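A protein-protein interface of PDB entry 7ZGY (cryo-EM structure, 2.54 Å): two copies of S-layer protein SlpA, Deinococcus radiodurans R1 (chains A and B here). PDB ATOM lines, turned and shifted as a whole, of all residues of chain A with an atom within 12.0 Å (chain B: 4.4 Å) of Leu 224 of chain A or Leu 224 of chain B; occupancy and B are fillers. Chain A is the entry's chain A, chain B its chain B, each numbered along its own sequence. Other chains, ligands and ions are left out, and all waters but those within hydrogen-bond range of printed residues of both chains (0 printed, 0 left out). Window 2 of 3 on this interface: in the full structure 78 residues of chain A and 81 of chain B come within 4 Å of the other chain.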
ATOM      1  N   SER A 219     -17.371  -4.394  16.153  1.00  0.00           N
ATOM      2  CA  SER A 219     -16.825  -5.706  15.827  1.00  0.00           C
ATOM      3  C   SER A 219     -17.918  -6.640  15.319  1.00  0.00           C
ATOM      4  O   SER A 219     -18.558  -6.365  14.306  1.00  0.00           O
ATOM      5  CB  SER A 219     -16.128  -6.316  17.044  1.00  0.00           C
ATOM      6  OG  SER A 219     -15.502  -7.544  16.713  1.00  0.00           O
ATOM      7  N   ASP A 220     -18.126  -7.748  16.029  1.00  0.00           N
ATOM      8  CA  ASP A 220     -19.119  -8.743  15.649  1.00  0.00           C
ATOM      9  C   ASP A 220     -20.411  -8.638  16.449  1.00  0.00           C
ATOM     10  O   ASP A 220     -21.309  -9.464  16.254  1.00  0.00           O
ATOM     11  CB  ASP A 220     -18.542 -10.155  15.798  1.00  0.00           C
ATOM     12  CG  ASP A 220     -18.161 -10.481  17.228  1.00  0.00           C
ATOM     13  OD1 ASP A 220     -18.285  -9.594  18.098  1.00  0.00           O
ATOM     14  OD2 ASP A 220     -17.742 -11.629  17.484  1.00  0.00           O
ATOM     15  N   PHE A 221     -20.530  -7.659  17.341  1.00  0.00           N
ATOM     16  CA  PHE A 221     -21.755  -7.489  18.112  1.00  0.00           C
ATOM     17  C   PHE A 221     -22.874  -6.820  17.323  1.00  0.00           C
ATOM     18  O   PHE A 221     -23.880  -6.427  17.921  1.00  0.00           O
ATOM     19  CB  PHE A 221     -21.477  -6.705  19.397  1.00  0.00           C
ATOM     20  CG  PHE A 221     -20.697  -7.479  20.423  1.00  0.00           C
ATOM     21  CD1 PHE A 221     -20.548  -8.851  20.303  1.00  0.00           C
ATOM     22  CD2 PHE A 221     -20.141  -6.844  21.519  1.00  0.00           C
ATOM     23  CE1 PHE A 221     -19.841  -9.572  21.247  1.00  0.00           C
ATOM     24  CE2 PHE A 221     -19.433  -7.560  22.466  1.00  0.00           C
ATOM     25  CZ  PHE A 221     -19.285  -8.925  22.330  1.00  0.00           C
ATOM     26  N   ASP A 222     -22.729  -6.679  16.004  1.00  0.00           N
ATOM     27  CA  ASP A 222     -23.866  -6.267  15.188  1.00  0.00           C
ATOM     28  C   ASP A 222     -24.980  -7.305  15.255  1.00  0.00           C
ATOM     29  O   ASP A 222     -26.162  -6.958  15.377  1.00  0.00           O
ATOM     30  CB  ASP A 222     -23.423  -6.045  13.742  1.00  0.00           C
ATOM     31  CG  ASP A 222     -22.178  -5.186  13.640  1.00  0.00           C
ATOM     32  OD1 ASP A 222     -21.070  -5.717  13.865  1.00  0.00           O
ATOM     33  OD2 ASP A 222     -22.307  -3.983  13.332  1.00  0.00           O
ATOM     34  N   ALA A 223     -24.616  -8.587  15.183  1.00  0.00           N
ATOM     35  CA  ALA A 223     -25.602  -9.646  15.356  1.00  0.00           C
ATOM     36  C   ALA A 223     -26.252  -9.565  16.731  1.00  0.00           C
ATOM     37  O   ALA A 223     -27.448  -9.841  16.877  1.00  0.00           O
ATOM     38  CB  ALA A 223     -24.948 -11.013  15.149  1.00  0.00           C
ATOM     39  N   LEU A 224     -25.479  -9.194  17.753  1.00  0.00           N
ATOM     40  CA  LEU A 224     -26.057  -9.015  19.079  1.00  0.00           C
ATOM     41  C   LEU A 224     -27.080  -7.886  19.081  1.00  0.00           C
ATOM     42  O   LEU A 224     -28.130  -7.991  19.725  1.00  0.00           O
ATOM     43  CB  LEU A 224     -24.954  -8.757  20.105  1.00  0.00           C
ATOM     44  CG  LEU A 224     -25.382  -8.725  21.573  1.00  0.00           C
ATOM     45  CD1 LEU A 224     -24.226  -9.116  22.476  1.00  0.00           C
ATOM     46  CD2 LEU A 224     -25.904  -7.349  21.949  1.00  0.00           C
ATOM     47  N   GLY A 225     -26.792  -6.796  18.369  1.00  0.00           N
ATOM     48  CA  GLY A 225     -27.773  -5.729  18.251  1.00  0.00           C
ATOM     49  C   GLY A 225     -29.035  -6.180  17.542  1.00  0.00           C
ATOM     50  O   GLY A 225     -30.147  -5.820  17.941  1.00  0.00           O
ATOM     51  N   GLY A 226     -28.883  -6.969  16.479  1.00  0.00           N
ATOM     52  CA  GLY A 226     -30.051  -7.520  15.814  1.00  0.00           C
ATOM     53  C   GLY A 226     -30.871  -8.410  16.729  1.00  0.00           C
ATOM     54  O   GLY A 226     -32.104  -8.361  16.722  1.00  0.00           O
ATOM     55  N   ARG A 227     -30.196  -9.235  17.531  1.00  0.00           N
ATOM     56  CA  ARG A 227     -30.897 -10.081  18.493  1.00  0.00           C
ATOM     57  C   ARG A 227     -31.627  -9.241  19.533  1.00  0.00           C
ATOM     58  O   ARG A 227     -32.745  -9.572  19.940  1.00  0.00           O
ATOM     59  CB  ARG A 227     -29.910 -11.035  19.166  1.00  0.00           C
ATOM     60  CG  ARG A 227     -29.185 -11.951  18.195  1.00  0.00           C
ATOM     61  CD  ARG A 227     -28.051 -12.704  18.872  1.00  0.00           C
ATOM     62  NE  ARG A 227     -28.542 -13.718  19.796  1.00  0.00           N
ATOM     63  CZ  ARG A 227     -28.309 -13.718  21.101  1.00  0.00           C
ATOM     64  NH1 ARG A 227     -27.586 -12.771  21.674  1.00  0.00           N
ATOM     65  NH2 ARG A 227     -28.815 -14.694  21.850  1.00  0.00           N
ATOM     66  N   VAL A 228     -31.004  -8.149  19.980  1.00  0.00           N
ATOM     67  CA  VAL A 228     -31.657  -7.261  20.938  1.00  0.00           C
ATOM     68  C   VAL A 228     -32.907  -6.645  20.324  1.00  0.00           C
ATOM     69  O   VAL A 228     -33.947  -6.532  20.981  1.00  0.00           O
ATOM     70  CB  VAL A 228     -30.676  -6.182  21.428  1.00  0.00           C
ATOM     71  CG1 VAL A 228     -31.427  -5.072  22.137  1.00  0.00           C
ATOM     72  CG2 VAL A 228     -29.644  -6.794  22.353  1.00  0.00           C
ATOM     73  N   THR A 229     -32.824  -6.227  19.061  1.00  0.00           N
ATOM     74  CA  THR A 229     -34.006  -5.686  18.391  1.00  0.00           C
ATOM     75  C   THR A 229     -35.102  -6.740  18.267  1.00  0.00           C
ATOM     76  O   THR A 229     -36.289  -6.444  18.467  1.00  0.00           O
ATOM     77  CB  THR A 229     -33.628  -5.140  17.016  1.00  0.00           C
ATOM     78  OG1 THR A 229     -32.586  -4.167  17.158  1.00  0.00           O
ATOM     79  CG2 THR A 229     -34.831  -4.492  16.355  1.00  0.00           C
ATOM     80  N   THR A 230     -34.723  -7.974  17.930  1.00  0.00           N
ATOM     81  CA  THR A 230     -35.708  -9.047  17.840  1.00  0.00           C
ATOM     82  C   THR A 230     -36.386  -9.280  19.182  1.00  0.00           C
ATOM     83  O   THR A 230     -37.601  -9.479  19.241  1.00  0.00           O
ATOM     84  CB  THR A 230     -35.055 -10.337  17.343  1.00  0.00           C
ATOM     85  OG1 THR A 230     -34.178 -10.852  18.352  1.00  0.00           O
ATOM     86  CG2 THR A 230     -34.275 -10.088  16.064  1.00  0.00           C
ATOM     87  N   VAL A 231     -35.615  -9.265  20.271  1.00  0.00           N
ATOM     88  CA  VAL A 231     -36.203  -9.431  21.599  1.00  0.00           C
ATOM     89  C   VAL A 231     -37.122  -8.262  21.925  1.00  0.00           C
ATOM     90  O   VAL A 231     -38.185  -8.436  22.534  1.00  0.00           O
ATOM     91  CB  VAL A 231     -35.103  -9.591  22.662  1.00  0.00           C
ATOM     92  CG1 VAL A 231     -35.706  -9.524  24.051  1.00  0.00           C
ATOM     93  CG2 VAL A 231     -34.369 -10.898  22.468  1.00  0.00           C
ATOM     94  N   GLU A 232     -36.719  -7.050  21.542  1.00  0.00           N
ATOM     95  CA  GLU A 232     -37.548  -5.876  21.794  1.00  0.00           C
ATOM     96  C   GLU A 232     -38.904  -6.018  21.119  1.00  0.00           C
ATOM     97  O   GLU A 232     -39.942  -5.695  21.705  1.00  0.00           O
ATOM     98  CB  GLU A 232     -36.834  -4.618  21.299  1.00  0.00           C
ATOM     99  CG  GLU A 232     -35.589  -4.246  22.083  1.00  0.00           C
ATOM    100  CD  GLU A 232     -35.910  -3.672  23.445  1.00  0.00           C
ATOM    101  OE1 GLU A 232     -37.020  -3.125  23.610  1.00  0.00           O
ATOM    102  OE2 GLU A 232     -35.053  -3.762  24.347  1.00  0.00           O
ATOM    103  N   THR A 233     -38.908  -6.494  19.873  1.00  0.00           N
ATOM    104  CA  THR A 233     -40.173  -6.698  19.171  1.00  0.00           C
ATOM    105  C   THR A 233     -40.950  -7.876  19.751  1.00  0.00           C
ATOM    106  O   THR A 233     -42.184  -7.835  19.836  1.00  0.00           O
ATOM    107  CB  THR A 233     -39.918  -6.907  17.681  1.00  0.00           C
ATOM    108  OG1 THR A 233     -39.338  -5.721  17.125  1.00  0.00           O
ATOM    109  CG2 THR A 233     -41.218  -7.214  16.958  1.00  0.00           C
ATOM    110  N   PHE B 221     -21.662   0.955  22.376  1.00  0.00           N
ATOM    111  CA  PHE B 221     -22.640  -0.021  22.843  1.00  0.00           C
ATOM    112  C   PHE B 221     -23.108   0.230  24.272  1.00  0.00           C
ATOM    113  O   PHE B 221     -23.801  -0.623  24.834  1.00  0.00           O
ATOM    114  CB  PHE B 221     -22.089  -1.444  22.719  1.00  0.00           C
ATOM    115  CG  PHE B 221     -21.923  -1.911  21.300  1.00  0.00           C
ATOM    116  CD1 PHE B 221     -22.525  -1.225  20.259  1.00  0.00           C
ATOM    117  CD2 PHE B 221     -21.200  -3.055  21.012  1.00  0.00           C
ATOM    118  CE1 PHE B 221     -22.387  -1.657  18.955  1.00  0.00           C
ATOM    119  CE2 PHE B 221     -21.060  -3.492  19.709  1.00  0.00           C
ATOM    120  CZ  PHE B 221     -21.654  -2.793  18.679  1.00  0.00           C
ATOM    121  N   ASP B 222     -22.753   1.367  24.874  1.00  0.00           N
ATOM    122  CA  ASP B 222     -23.357   1.728  26.151  1.00  0.00           C
ATOM    123  C   ASP B 222     -24.864   1.893  26.004  1.00  0.00           C
ATOM    124  O   ASP B 222     -25.638   1.432  26.854  1.00  0.00           O
ATOM    125  CB  ASP B 222     -22.724   3.010  26.690  1.00  0.00           C
ATOM    126  CG  ASP B 222     -21.209   2.971  26.653  1.00  0.00           C
ATOM    127  OD1 ASP B 222     -20.636   3.183  25.565  1.00  0.00           O
ATOM    128  OD2 ASP B 222     -20.593   2.731  27.713  1.00  0.00           O
ATOM    129  N   ALA B 223     -25.299   2.547  24.924  1.00  0.00           N
ATOM    130  CA  ALA B 223     -26.726   2.634  24.640  1.00  0.00           C
ATOM    131  C   ALA B 223     -27.333   1.249  24.469  1.00  0.00           C
ATOM    132  O   ALA B 223     -28.492   1.020  24.834  1.00  0.00           O
ATOM    133  CB  ALA B 223     -26.962   3.486  23.392  1.00  0.00           C
ATOM    134  N   LEU B 224     -26.565   0.308  23.915  1.00  0.00           N
ATOM    135  CA  LEU B 224     -27.052  -1.062  23.808  1.00  0.00           C
ATOM    136  C   LEU B 224     -27.284  -1.667  25.186  1.00  0.00           C
ATOM    137  O   LEU B 224     -28.282  -2.361  25.407  1.00  0.00           O
ATOM    138  CB  LEU B 224     -26.069  -1.911  23.004  1.00  0.00           C
ATOM    139  CG  LEU B 224     -26.622  -3.245  22.501  1.00  0.00           C
ATOM    140  CD1 LEU B 224     -27.718  -3.012  21.477  1.00  0.00           C
ATOM    141  CD2 LEU B 224     -25.516  -4.106  21.918  1.00  0.00           C
ATOM    142  N   GLY B 225     -26.372  -1.417  26.126  1.00  0.00           N
ATOM    143  CA  GLY B 225     -26.584  -1.891  27.484  1.00  0.00           C
ATOM    144  C   GLY B 225     -27.802  -1.260  28.131  1.00  0.00           C
ATOM    145  O   GLY B 225     -28.557  -1.928  28.843  1.00  0.00           O
ATOM    146  N   GLY B 226     -28.009   0.036  27.894  1.00  0.00           N
ATOM    147  CA  GLY B 226     -29.211   0.678  28.399  1.00  0.00           C
ATOM    148  C   GLY B 226     -30.477   0.064  27.832  1.00  0.00           C
ATOM    149  O   GLY B 226     -31.452  -0.159  28.555  1.00  0.00           O
ATOM    150  N   ARG B 227     -30.478  -0.221  26.528  1.00  0.00           N
ATOM    151  CA  ARG B 227     -31.629  -0.869  25.907  1.00  0.00           C
ATOM    152  C   ARG B 227     -31.852  -2.260  26.486  1.00  0.00           C
ATOM    153  O   ARG B 227     -32.997  -2.680  26.695  1.00  0.00           O
ATOM    154  CB  ARG B 227     -31.433  -0.941  24.393  1.00  0.00           C
ATOM    155  CG  ARG B 227     -31.239   0.412  23.733  1.00  0.00           C
ATOM    156  CD  ARG B 227     -30.816   0.272  22.280  1.00  0.00           C
ATOM    157  NE  ARG B 227     -31.897  -0.224  21.438  1.00  0.00           N
ATOM    158  CZ  ARG B 227     -31.861  -1.369  20.770  1.00  0.00           C
ATOM    159  NH1 ARG B 227     -30.804  -2.160  20.811  1.00  0.00           N
ATOM    160  NH2 ARG B 227     -32.913  -1.726  20.038  1.00  0.00           N
ATOM    161  N   VAL B 228     -30.768  -2.996  26.741  1.00  0.00           N
ATOM    162  CA  VAL B 228     -30.894  -4.320  27.339  1.00  0.00           C
ATOM    163  C   VAL B 228     -31.513  -4.220  28.726  1.00  0.00           C
ATOM    164  O   VAL B 228     -32.374  -5.025  29.095  1.00  0.00           O
ATOM    165  CB  VAL B 228     -29.527  -5.027  27.380  1.00  0.00           C
ATOM    166  CG1 VAL B 228     -29.578  -6.217  28.317  1.00  0.00           C
ATOM    167  CG2 VAL B 228     -29.123  -5.469  25.987  1.00  0.00           C
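OE2 of Glu 232 of chain A lies close to O of Arg 227 of chain B, at 3.3 Å.
The backbone carbonyl oxygen (O) of Gly 225 of chain A sits at hydrogen-bond distance from the side-chain hydroxyl (OG1) of Thr 229 of chain A (3.0 Å).
O of Thr 229 of chain A is in hydrogen-bond range of OG1 of Thr 233 of chain A (3.4 Å).
Among the printed residues, pairs that only touch across the chains: Phe 221 of chain A with Phe 221 of chain B (3.3 Å), Val 228 of chain A with Arg 227 of chain B (3.3 Å), Leu 224 of chain A with Leu 224 of chain B (3.3 Å), Thr 229 of chain A with Arg 227 of chain B (3.8 Å) and Val 228 of chain A with Val 228 of chain B (3.9 Å).
Printed residues of chain B within 4 Å of Phe 221 of chain A: Phe 221 (3.3 Å).
Asp 222 of chain A touches none of the printed residues of chain B.
Ala 223 of chain A touches none of the printed residues of chain B.
Of the printed residues of chain B, Leu 224 of chain A touches Leu 224.
Of the printed residues of chain B, Val 228 of chain A touches Arg 227 and Val 228.
Printed residues of chain B within 4 Å of Thr 229 of chain A: Arg 227 (3.8 Å).
Printed residues of chain B within 4 Å of Glu 232 of chain A: Arg 227 (3.3 Å).
Phe 221 of chain B touches just one residue of chain A: Phe 221.
Ala 223 of chain B touches none of the printed residues of chain A.
Of the printed residues of chain A, Leu 224 of chain B touches Leu 224.
Gly 225 of chain B touches none of the printed residues of chain A.
No residue of chain A comes within 4 Å of Gly 226 of chain B.
The nearest printed residue of chain B that does not touch Thr 229 of chain A is Leu 224 of chain B (6.5 Å).
Hydrophobic or aromatic side chains of chain A within 4 Å of the printed part of chain B: Phe 221, Leu 224 and Val 228.
Of the 8 printed residues of chain B, 4 touch a printed residue of chain A.
Printed residues of chain B that touch a printed residue of chain A: Phe 221, Leu 224, Arg 227 and Val 228.
Hydrophobic or aromatic side chains of chain B within 4 Å of the printed part of chain A: Phe 221, Leu 224 and Val 228.
Among the printed residues, no Asp or Glu carboxylate lies within 4 Å of a Lys or Arg side-chain nitrogen of the other chain.
Phe 221 of chain B touches its own counterpart, Phe 221 of chain A.
Leu 224 of chain B touches its own counterpart, Leu 224 of chain A.
Val 228 of chain A touches Arg 227 of chain B, but with the chains exchanged Arg 227 of chain A does not touch Val 228 of chain B (7.9 Å).
Val 228 of chain A touches its own counterpart, Val 228 of chain B.
8 positions are printed for both chains.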
